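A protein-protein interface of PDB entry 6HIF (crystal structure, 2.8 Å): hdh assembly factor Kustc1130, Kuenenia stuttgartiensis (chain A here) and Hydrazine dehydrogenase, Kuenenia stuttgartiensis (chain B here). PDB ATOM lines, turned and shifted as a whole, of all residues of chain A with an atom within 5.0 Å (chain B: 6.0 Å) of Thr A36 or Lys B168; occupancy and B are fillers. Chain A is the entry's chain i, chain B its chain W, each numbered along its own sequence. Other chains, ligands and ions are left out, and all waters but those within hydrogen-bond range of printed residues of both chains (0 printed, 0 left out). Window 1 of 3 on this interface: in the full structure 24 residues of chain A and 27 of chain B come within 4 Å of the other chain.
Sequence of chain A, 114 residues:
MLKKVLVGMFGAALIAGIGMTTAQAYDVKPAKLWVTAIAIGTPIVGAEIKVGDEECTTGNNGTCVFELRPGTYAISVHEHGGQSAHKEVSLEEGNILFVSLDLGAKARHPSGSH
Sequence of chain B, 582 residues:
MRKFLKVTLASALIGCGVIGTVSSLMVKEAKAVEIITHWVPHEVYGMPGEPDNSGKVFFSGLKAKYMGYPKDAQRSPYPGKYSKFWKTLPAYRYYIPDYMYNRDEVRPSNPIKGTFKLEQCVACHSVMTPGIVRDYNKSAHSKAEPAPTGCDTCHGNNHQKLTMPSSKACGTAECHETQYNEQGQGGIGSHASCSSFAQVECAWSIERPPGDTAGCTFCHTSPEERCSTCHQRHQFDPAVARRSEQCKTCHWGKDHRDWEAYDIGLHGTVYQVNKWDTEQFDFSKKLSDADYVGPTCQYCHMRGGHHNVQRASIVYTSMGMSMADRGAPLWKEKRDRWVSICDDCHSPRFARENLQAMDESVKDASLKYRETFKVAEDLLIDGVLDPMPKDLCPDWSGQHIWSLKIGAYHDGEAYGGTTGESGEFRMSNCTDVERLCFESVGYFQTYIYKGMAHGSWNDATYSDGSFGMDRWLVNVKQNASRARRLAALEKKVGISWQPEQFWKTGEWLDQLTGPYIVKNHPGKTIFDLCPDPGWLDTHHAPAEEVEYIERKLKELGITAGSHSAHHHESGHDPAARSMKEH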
ATOM      1  N   TRP A  34     -18.057 -27.839  10.879  1.00  0.00           N
ATOM      2  CA  TRP A  34     -19.338 -27.329  10.421  1.00  0.00           C
ATOM      3  C   TRP A  34     -19.696 -26.106  11.260  1.00  0.00           C
ATOM      4  O   TRP A  34     -19.640 -26.160  12.487  1.00  0.00           O
ATOM      5  CB  TRP A  34     -20.421 -28.407  10.556  1.00  0.00           C
ATOM      6  CG  TRP A  34     -20.158 -29.697   9.839  1.00  0.00           C
ATOM      7  CD1 TRP A  34     -19.117 -30.559  10.034  1.00  0.00           C
ATOM      8  CD2 TRP A  34     -20.993 -30.302   8.836  1.00  0.00           C
ATOM      9  NE1 TRP A  34     -19.232 -31.644   9.207  1.00  0.00           N
ATOM     10  CE2 TRP A  34     -20.374 -31.516   8.462  1.00  0.00           C
ATOM     11  CE3 TRP A  34     -22.192 -29.935   8.215  1.00  0.00           C
ATOM     12  CZ2 TRP A  34     -20.919 -32.357   7.492  1.00  0.00           C
ATOM     13  CZ3 TRP A  34     -22.729 -30.769   7.257  1.00  0.00           C
ATOM     14  CH2 TRP A  34     -22.099 -31.963   6.904  1.00  0.00           C
ATOM     15  N   VAL A  35     -20.058 -25.006  10.590  1.00  0.00           N
ATOM     16  CA  VAL A  35     -20.510 -23.813  11.290  1.00  0.00           C
ATOM     17  C   VAL A  35     -21.896 -23.433  10.773  1.00  0.00           C
ATOM     18  O   VAL A  35     -22.063 -23.150   9.589  1.00  0.00           O
ATOM     19  CB  VAL A  35     -19.509 -22.645  11.174  1.00  0.00           C
ATOM     20  CG1 VAL A  35     -19.969 -21.431  11.967  1.00  0.00           C
ATOM     21  CG2 VAL A  35     -18.106 -23.049  11.603  1.00  0.00           C
ATOM     22  N   THR A  36     -22.876 -23.434  11.685  1.00  0.00           N
ATOM     23  CA  THR A  36     -24.256 -23.095  11.371  1.00  0.00           C
ATOM     24  C   THR A  36     -24.592 -21.733  11.972  1.00  0.00           C
ATOM     25  O   THR A  36     -24.388 -21.506  13.165  1.00  0.00           O
ATOM     26  CB  THR A  36     -25.222 -24.195  11.839  1.00  0.00           C
ATOM     27  OG1 THR A  36     -24.782 -25.442  11.300  1.00  0.00           O
ATOM     28  CG2 THR A  36     -26.658 -23.947  11.430  1.00  0.00           C
ATOM     29  N   ALA A  37     -25.110 -20.837  11.120  1.00  0.00           N
ATOM     30  CA  ALA A  37     -25.530 -19.504  11.519  1.00  0.00           C
ATOM     31  C   ALA A  37     -27.046 -19.482  11.702  1.00  0.00           C
ATOM     32  O   ALA A  37     -27.796 -19.710  10.754  1.00  0.00           O
ATOM     33  CB  ALA A  37     -25.077 -18.493  10.492  1.00  0.00           C
ATOM     34  N   ILE A  38     -27.477 -19.209  12.939  1.00  0.00           N
ATOM     35  CA  ILE A  38     -28.885 -19.224  13.297  1.00  0.00           C
ATOM     36  C   ILE A  38     -29.299 -17.833  13.773  1.00  0.00           C
ATOM     37  O   ILE A  38     -28.503 -17.109  14.371  1.00  0.00           O
ATOM     38  CB  ILE A  38     -29.181 -20.286  14.379  1.00  0.00           C
ATOM     39  CG1 ILE A  38     -28.276 -21.516  14.281  1.00  0.00           C
ATOM     40  CG2 ILE A  38     -30.648 -20.675  14.358  1.00  0.00           C
ATOM     41  CD1 ILE A  38     -28.379 -22.433  15.480  1.00  0.00           C
ATOM     42  N   GLY A  41     -33.365 -19.737  15.763  1.00  0.00           N
ATOM     43  CA  GLY A  41     -33.952 -20.955  15.227  1.00  0.00           C
ATOM     44  C   GLY A  41     -33.811 -21.079  13.712  1.00  0.00           C
ATOM     45  O   GLY A  41     -33.530 -22.162  13.203  1.00  0.00           O
ATOM     46  N   PRO A  43     -32.228 -20.440   9.914  1.00  0.00           N
ATOM     47  CA  PRO A  43     -30.908 -20.257   9.304  1.00  0.00           C
ATOM     48  C   PRO A  43     -30.738 -18.888   8.648  1.00  0.00           C
ATOM     49  O   PRO A  43     -31.657 -18.387   8.002  1.00  0.00           O
ATOM     50  CB  PRO A  43     -30.850 -21.352   8.229  1.00  0.00           C
ATOM     51  CG  PRO A  43     -32.299 -21.650   7.904  1.00  0.00           C
ATOM     52  CD  PRO A  43     -33.038 -21.449   9.210  1.00  0.00           C
ATOM     53  N   ASN A  61     -28.831 -23.380   3.842  1.00  0.00           N
ATOM     54  CA  ASN A  61     -28.481 -24.130   5.038  1.00  0.00           C
ATOM     55  C   ASN A  61     -28.212 -23.176   6.194  1.00  0.00           C
ATOM     56  O   ASN A  61     -28.571 -23.460   7.333  1.00  0.00           O
ATOM     57  CB  ASN A  61     -27.143 -24.857   4.895  1.00  0.00           C
ATOM     58  CG  ASN A  61     -27.131 -25.968   3.872  1.00  0.00           C
ATOM     59  OD1 ASN A  61     -27.532 -25.775   2.728  1.00  0.00           O
ATOM     60  ND2 ASN A  61     -26.639 -27.129   4.273  1.00  0.00           N
ATOM     61  N   GLY A  62     -27.530 -22.068   5.884  1.00  0.00           N
ATOM     62  CA  GLY A  62     -26.882 -21.254   6.896  1.00  0.00           C
ATOM     63  C   GLY A  62     -25.670 -21.974   7.481  1.00  0.00           C
ATOM     64  O   GLY A  62     -25.178 -21.604   8.543  1.00  0.00           O
ATOM     65  N   THR A  63     -25.198 -23.002   6.763  1.00  0.00           N
ATOM     66  CA  THR A  63     -24.131 -23.869   7.236  1.00  0.00           C
ATOM     67  C   THR A  63     -22.982 -23.876   6.231  1.00  0.00           C
ATOM     68  O   THR A  63     -23.197 -24.046   5.033  1.00  0.00           O
ATOM     69  CB  THR A  63     -24.650 -25.282   7.533  1.00  0.00           C
ATOM     70  OG1 THR A  63     -25.766 -25.164   8.416  1.00  0.00           O
ATOM     71  CG2 THR A  63     -23.608 -26.185   8.154  1.00  0.00           C
ATOM     72  N   VAL A  99     -20.417 -26.623  14.996  1.00  0.00           N
ATOM     73  CA  VAL A  99     -20.551 -25.424  15.807  1.00  0.00           C
ATOM     74  C   VAL A  99     -21.827 -24.699  15.388  1.00  0.00           C
ATOM     75  O   VAL A  99     -22.057 -24.471  14.202  1.00  0.00           O
ATOM     76  CB  VAL A  99     -19.303 -24.523  15.703  1.00  0.00           C
ATOM     77  CG1 VAL A  99     -19.541 -23.138  16.288  1.00  0.00           C
ATOM     78  CG2 VAL A  99     -18.088 -25.167  16.351  1.00  0.00           C
ATOM     79  N   SER A 100     -22.653 -24.361  16.383  1.00  0.00           N
ATOM     80  CA  SER A 100     -23.914 -23.680  16.154  1.00  0.00           C
ATOM     81  C   SER A 100     -23.907 -22.344  16.892  1.00  0.00           C
ATOM     82  O   SER A 100     -23.858 -22.311  18.121  1.00  0.00           O
ATOM     83  CB  SER A 100     -25.064 -24.543  16.588  1.00  0.00           C
ATOM     84  OG  SER A 100     -26.196 -24.313  15.768  1.00  0.00           O
ATOM     85  N   LEU A 101     -23.940 -21.252  16.118  1.00  0.00           N
ATOM     86  CA  LEU A 101     -23.881 -19.906  16.666  1.00  0.00           C
ATOM     87  C   LEU A 101     -25.165 -19.154  16.325  1.00  0.00           C
ATOM     88  O   LEU A 101     -25.522 -19.022  15.155  1.00  0.00           O
ATOM     89  CB  LEU A 101     -22.649 -19.184  16.108  1.00  0.00           C
ATOM     90  CG  LEU A 101     -21.294 -19.752  16.533  1.00  0.00           C
ATOM     91  CD1 LEU A 101     -20.187 -19.243  15.622  1.00  0.00           C
ATOM     92  CD2 LEU A 101     -20.984 -19.425  17.988  1.00  0.00           C
ATOM     93  N   ASP B  98     -30.318 -27.800  15.858  1.00  0.00           N
ATOM     94  CA  ASP B  98     -29.332 -26.768  15.580  1.00  0.00           C
ATOM     95  C   ASP B  98     -29.328 -25.735  16.703  1.00  0.00           C
ATOM     96  O   ASP B  98     -28.268 -25.327  17.172  1.00  0.00           O
ATOM     97  CB  ASP B  98     -29.569 -26.117  14.215  1.00  0.00           C
ATOM     98  CG  ASP B  98     -29.030 -26.935  13.056  1.00  0.00           C
ATOM     99  OD1 ASP B  98     -28.001 -27.618  13.245  1.00  0.00           O
ATOM    100  OD2 ASP B  98     -29.643 -26.879  11.974  1.00  0.00           O
ATOM    101  N   PRO B 165     -27.551 -34.118  13.969  1.00  0.00           N
ATOM    102  CA  PRO B 165     -27.576 -33.562  12.617  1.00  0.00           C
ATOM    103  C   PRO B 165     -28.986 -33.218  12.145  1.00  0.00           C
ATOM    104  O   PRO B 165     -29.862 -34.081  12.072  1.00  0.00           O
ATOM    105  CB  PRO B 165     -26.960 -34.681  11.765  1.00  0.00           C
ATOM    106  CG  PRO B 165     -27.289 -35.960  12.513  1.00  0.00           C
ATOM    107  CD  PRO B 165     -27.414 -35.582  13.976  1.00  0.00           C
ATOM    108  N   SER B 166     -29.183 -31.935  11.823  1.00  0.00           N
ATOM    109  CA  SER B 166     -30.455 -31.454  11.314  1.00  0.00           C
ATOM    110  C   SER B 166     -30.512 -31.671   9.807  1.00  0.00           C
ATOM    111  O   SER B 166     -29.605 -32.263   9.229  1.00  0.00           O
ATOM    112  CB  SER B 166     -30.650 -30.004  11.654  1.00  0.00           C
ATOM    113  OG  SER B 166     -29.855 -29.183  10.809  1.00  0.00           O
ATOM    114  N   SER B 167     -31.583 -31.165   9.184  1.00  0.00           N
ATOM    115  CA  SER B 167     -31.752 -31.218   7.740  1.00  0.00           C
ATOM    116  C   SER B 167     -30.648 -30.425   7.044  1.00  0.00           C
ATOM    117  O   SER B 167     -30.287 -30.732   5.910  1.00  0.00           O
ATOM    118  CB  SER B 167     -33.120 -30.734   7.340  1.00  0.00           C
ATOM    119  OG  SER B 167     -33.443 -29.527   8.016  1.00  0.00           O
ATOM    120  N   LYS B 168     -30.112 -29.415   7.741  1.00  0.00           N
ATOM    121  CA  LYS B 168     -29.045 -28.579   7.217  1.00  0.00           C
ATOM    122  C   LYS B 168     -27.766 -29.402   7.073  1.00  0.00           C
ATOM    123  O   LYS B 168     -26.993 -29.192   6.139  1.00  0.00           O
ATOM    124  CB  LYS B 168     -28.808 -27.370   8.127  1.00  0.00           C
ATOM    125  CG  LYS B 168     -29.985 -26.416   8.268  1.00  0.00           C
ATOM    126  CD  LYS B 168     -29.703 -25.276   9.223  1.00  0.00           C
ATOM    127  CE  LYS B 168     -30.959 -24.628   9.766  1.00  0.00           C
ATOM    128  NZ  LYS B 168     -31.696 -25.544  10.667  1.00  0.00           N
ATOM    129  N   ALA B 169     -27.559 -30.335   8.011  1.00  0.00           N
ATOM    130  CA  ALA B 169     -26.376 -31.180   8.024  1.00  0.00           C
ATOM    131  C   ALA B 169     -26.415 -32.146   6.842  1.00  0.00           C
ATOM    132  O   ALA B 169     -25.401 -32.350   6.179  1.00  0.00           O
ATOM    133  CB  ALA B 169     -26.270 -31.909   9.342  1.00  0.00           C
ATOM    134  N   CYS B 170     -27.597 -32.719   6.587  1.00  0.00           N
ATOM    135  CA  CYS B 170     -27.785 -33.661   5.495  1.00  0.00           C
ATOM    136  C   CYS B 170     -27.701 -32.921   4.164  1.00  0.00           C
ATOM    137  O   CYS B 170     -27.235 -33.478   3.173  1.00  0.00           O
ATOM    138  CB  CYS B 170     -29.154 -34.330   5.559  1.00  0.00           C
ATOM    139  SG  CYS B 170     -29.531 -35.138   7.136  1.00  0.00           S
ATOM    140  N   GLY B 171     -28.156 -31.662   4.165  1.00  0.00           N
ATOM    141  CA  GLY B 171     -28.404 -30.917   2.941  1.00  0.00           C
ATOM    142  C   GLY B 171     -27.211 -30.078   2.492  1.00  0.00           C
ATOM    143  O   GLY B 171     -27.365 -29.167   1.680  1.00  0.00           O
ATOM    144  N   THR B 172     -26.026 -30.400   3.022  1.00  0.00           N
ATOM    145  CA  THR B 172     -24.800 -29.733   2.622  1.00  0.00           C
ATOM    146  C   THR B 172     -24.526 -30.041   1.153  1.00  0.00           C
ATOM    147  O   THR B 172     -24.945 -31.081   0.651  1.00  0.00           O
ATOM    148  CB  THR B 172     -23.646 -30.064   3.579  1.00  0.00           C
ATOM    149  OG1 THR B 172     -22.503 -29.319   3.160  1.00  0.00           O
ATOM    150  CG2 THR B 172     -23.299 -31.535   3.622  1.00  0.00           C
ATOM    151  N   TYR B 180     -32.631 -31.362   0.089  1.00  0.00           N
ATOM    152  CA  TYR B 180     -32.869 -30.269   1.017  1.00  0.00           C
ATOM    153  C   TYR B 180     -33.543 -29.106   0.292  1.00  0.00           C
ATOM    154  O   TYR B 180     -34.533 -28.559   0.779  1.00  0.00           O
ATOM    155  CB  TYR B 180     -31.565 -29.820   1.679  1.00  0.00           C
ATOM    156  CG  TYR B 180     -31.736 -28.733   2.711  1.00  0.00           C
ATOM    157  CD1 TYR B 180     -32.230 -29.021   3.973  1.00  0.00           C
ATOM    158  CD2 TYR B 180     -31.411 -27.414   2.428  1.00  0.00           C
ATOM    159  CE1 TYR B 180     -32.396 -28.030   4.929  1.00  0.00           C
ATOM    160  CE2 TYR B 180     -31.568 -26.411   3.372  1.00  0.00           C
ATOM    161  CZ  TYR B 180     -32.063 -26.720   4.629  1.00  0.00           C
ATOM    162  OH  TYR B 180     -32.220 -25.746   5.572  1.00  0.00           O
ATOM    163  N   GLU B 225     -36.937 -30.468  10.192  1.00  0.00           N
ATOM    164  CA  GLU B 225     -35.701 -30.376  10.955  1.00  0.00           C
ATOM    165  C   GLU B 225     -34.888 -31.666  10.867  1.00  0.00           C
ATOM    166  O   GLU B 225     -33.660 -31.619  10.918  1.00  0.00           O
ATOM    167  CB  GLU B 225     -35.993 -29.999  12.409  1.00  0.00           C
ATOM    168  CG  GLU B 225     -36.409 -28.550  12.594  1.00  0.00           C
ATOM    169  CD  GLU B 225     -35.349 -27.500  12.292  1.00  0.00           C
ATOM    170  OE1 GLU B 225     -35.733 -26.355  11.988  1.00  0.00           O
ATOM    171  OE2 GLU B 225     -34.144 -27.823  12.368  1.00  0.00           O
ATOM    172  N   CYS B 227     -34.186 -35.350   8.845  1.00  0.00           N
ATOM    173  CA  CYS B 227     -34.336 -36.080   7.596  1.00  0.00           C
ATOM    174  C   CYS B 227     -34.414 -37.586   7.849  1.00  0.00           C
ATOM    175  O   CYS B 227     -34.420 -38.374   6.906  1.00  0.00           O
ATOM    176  CB  CYS B 227     -33.195 -35.752   6.642  1.00  0.00           C
ATOM    177  SG  CYS B 227     -33.262 -34.054   6.016  1.00  0.00           S
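Printed residues of chain B within 4 Å of Thr A36: Lys B168 (3.99 Å). Of the printed residues of chain B, Ile A38 touches Asp B98 (3.4 Å). Printed residues of chain B within 4 Å of Thr A63: Lys B168 (3.8 Å). Of the printed residues of chain B, Ser A100 touches Asp B98 (2.7 Å). Of the printed residues of chain A, Lys B168 touches Thr A36 (3.99 Å), Pro A43 (3.6 Å), Asn A61 (2.8 Å) and Thr A63 (3.8 Å). The nearest printed residue of chain A that does not touch Thr B172 is Thr A63 (5.6 Å).
N of Lys B168 sits close to OG of Ser B166, 3.1 Å away. The backbone carbonyl oxygen (O) of Thr A36 is in hydrogen-bond range of the backbone NH (N) of Leu A101, 3.0 Å away. The side-chain carboxylate (OE2) of Glu B225 lies within salt-bridge range of the side-chain amino group (NZ) of Lys B168 (3.8 Å). O of Leu A101 is in hydrogen-bond range of N of Ile A38 (3.0 Å). OD2 of Asp B98 is in salt-bridge range of NZ of Lys B168 (2.8 Å). The backbone carbonyl oxygen (O) of Val A99 sits at hydrogen-bond distance from the backbone NH (N) of Thr A36 (2.8 Å).
The side-chain hydroxyl (OG) of Ser A100 lies within hydrogen-bond range of the backbone carbonyl oxygen (O) of Asp B98 (2.7 Å). The side-chain amide nitrogen (ND2) of Asn A61 lies within hydrogen-bond range of the backbone carbonyl oxygen (O) of Gly B171, 3.4 Å away. The side-chain amide nitrogen (ND2) of Asn A61 is in hydrogen-bond range of the backbone carbonyl oxygen (O) of Lys B168.
Of the 12 printed residues of chain B, 5 touch a printed residue of chain A. Of the 13 printed residues of chain A, 7 touch a printed residue of chain B. Hydrophobic or aromatic side chains of chain A within 4 Å of the printed part of chain B: Trp A34, Ile A38 and Pro A43. Among the printed residues, 10 pairs touch across the chains.
Among the printed residues, pairs that only touch across the chains: Trp A34 with Ala B169 (3.3 Å), Trp A34 with Thr B172 (3.5 Å), Thr A36 with Lys B168 (3.99 Å), Ile A38 with Asp B98 (3.4 Å), Pro A43 with Lys B168 (3.6 Å), Asn A61 with Thr B172 (3.6 Å) and Thr A63 with Lys B168 (3.8 Å).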
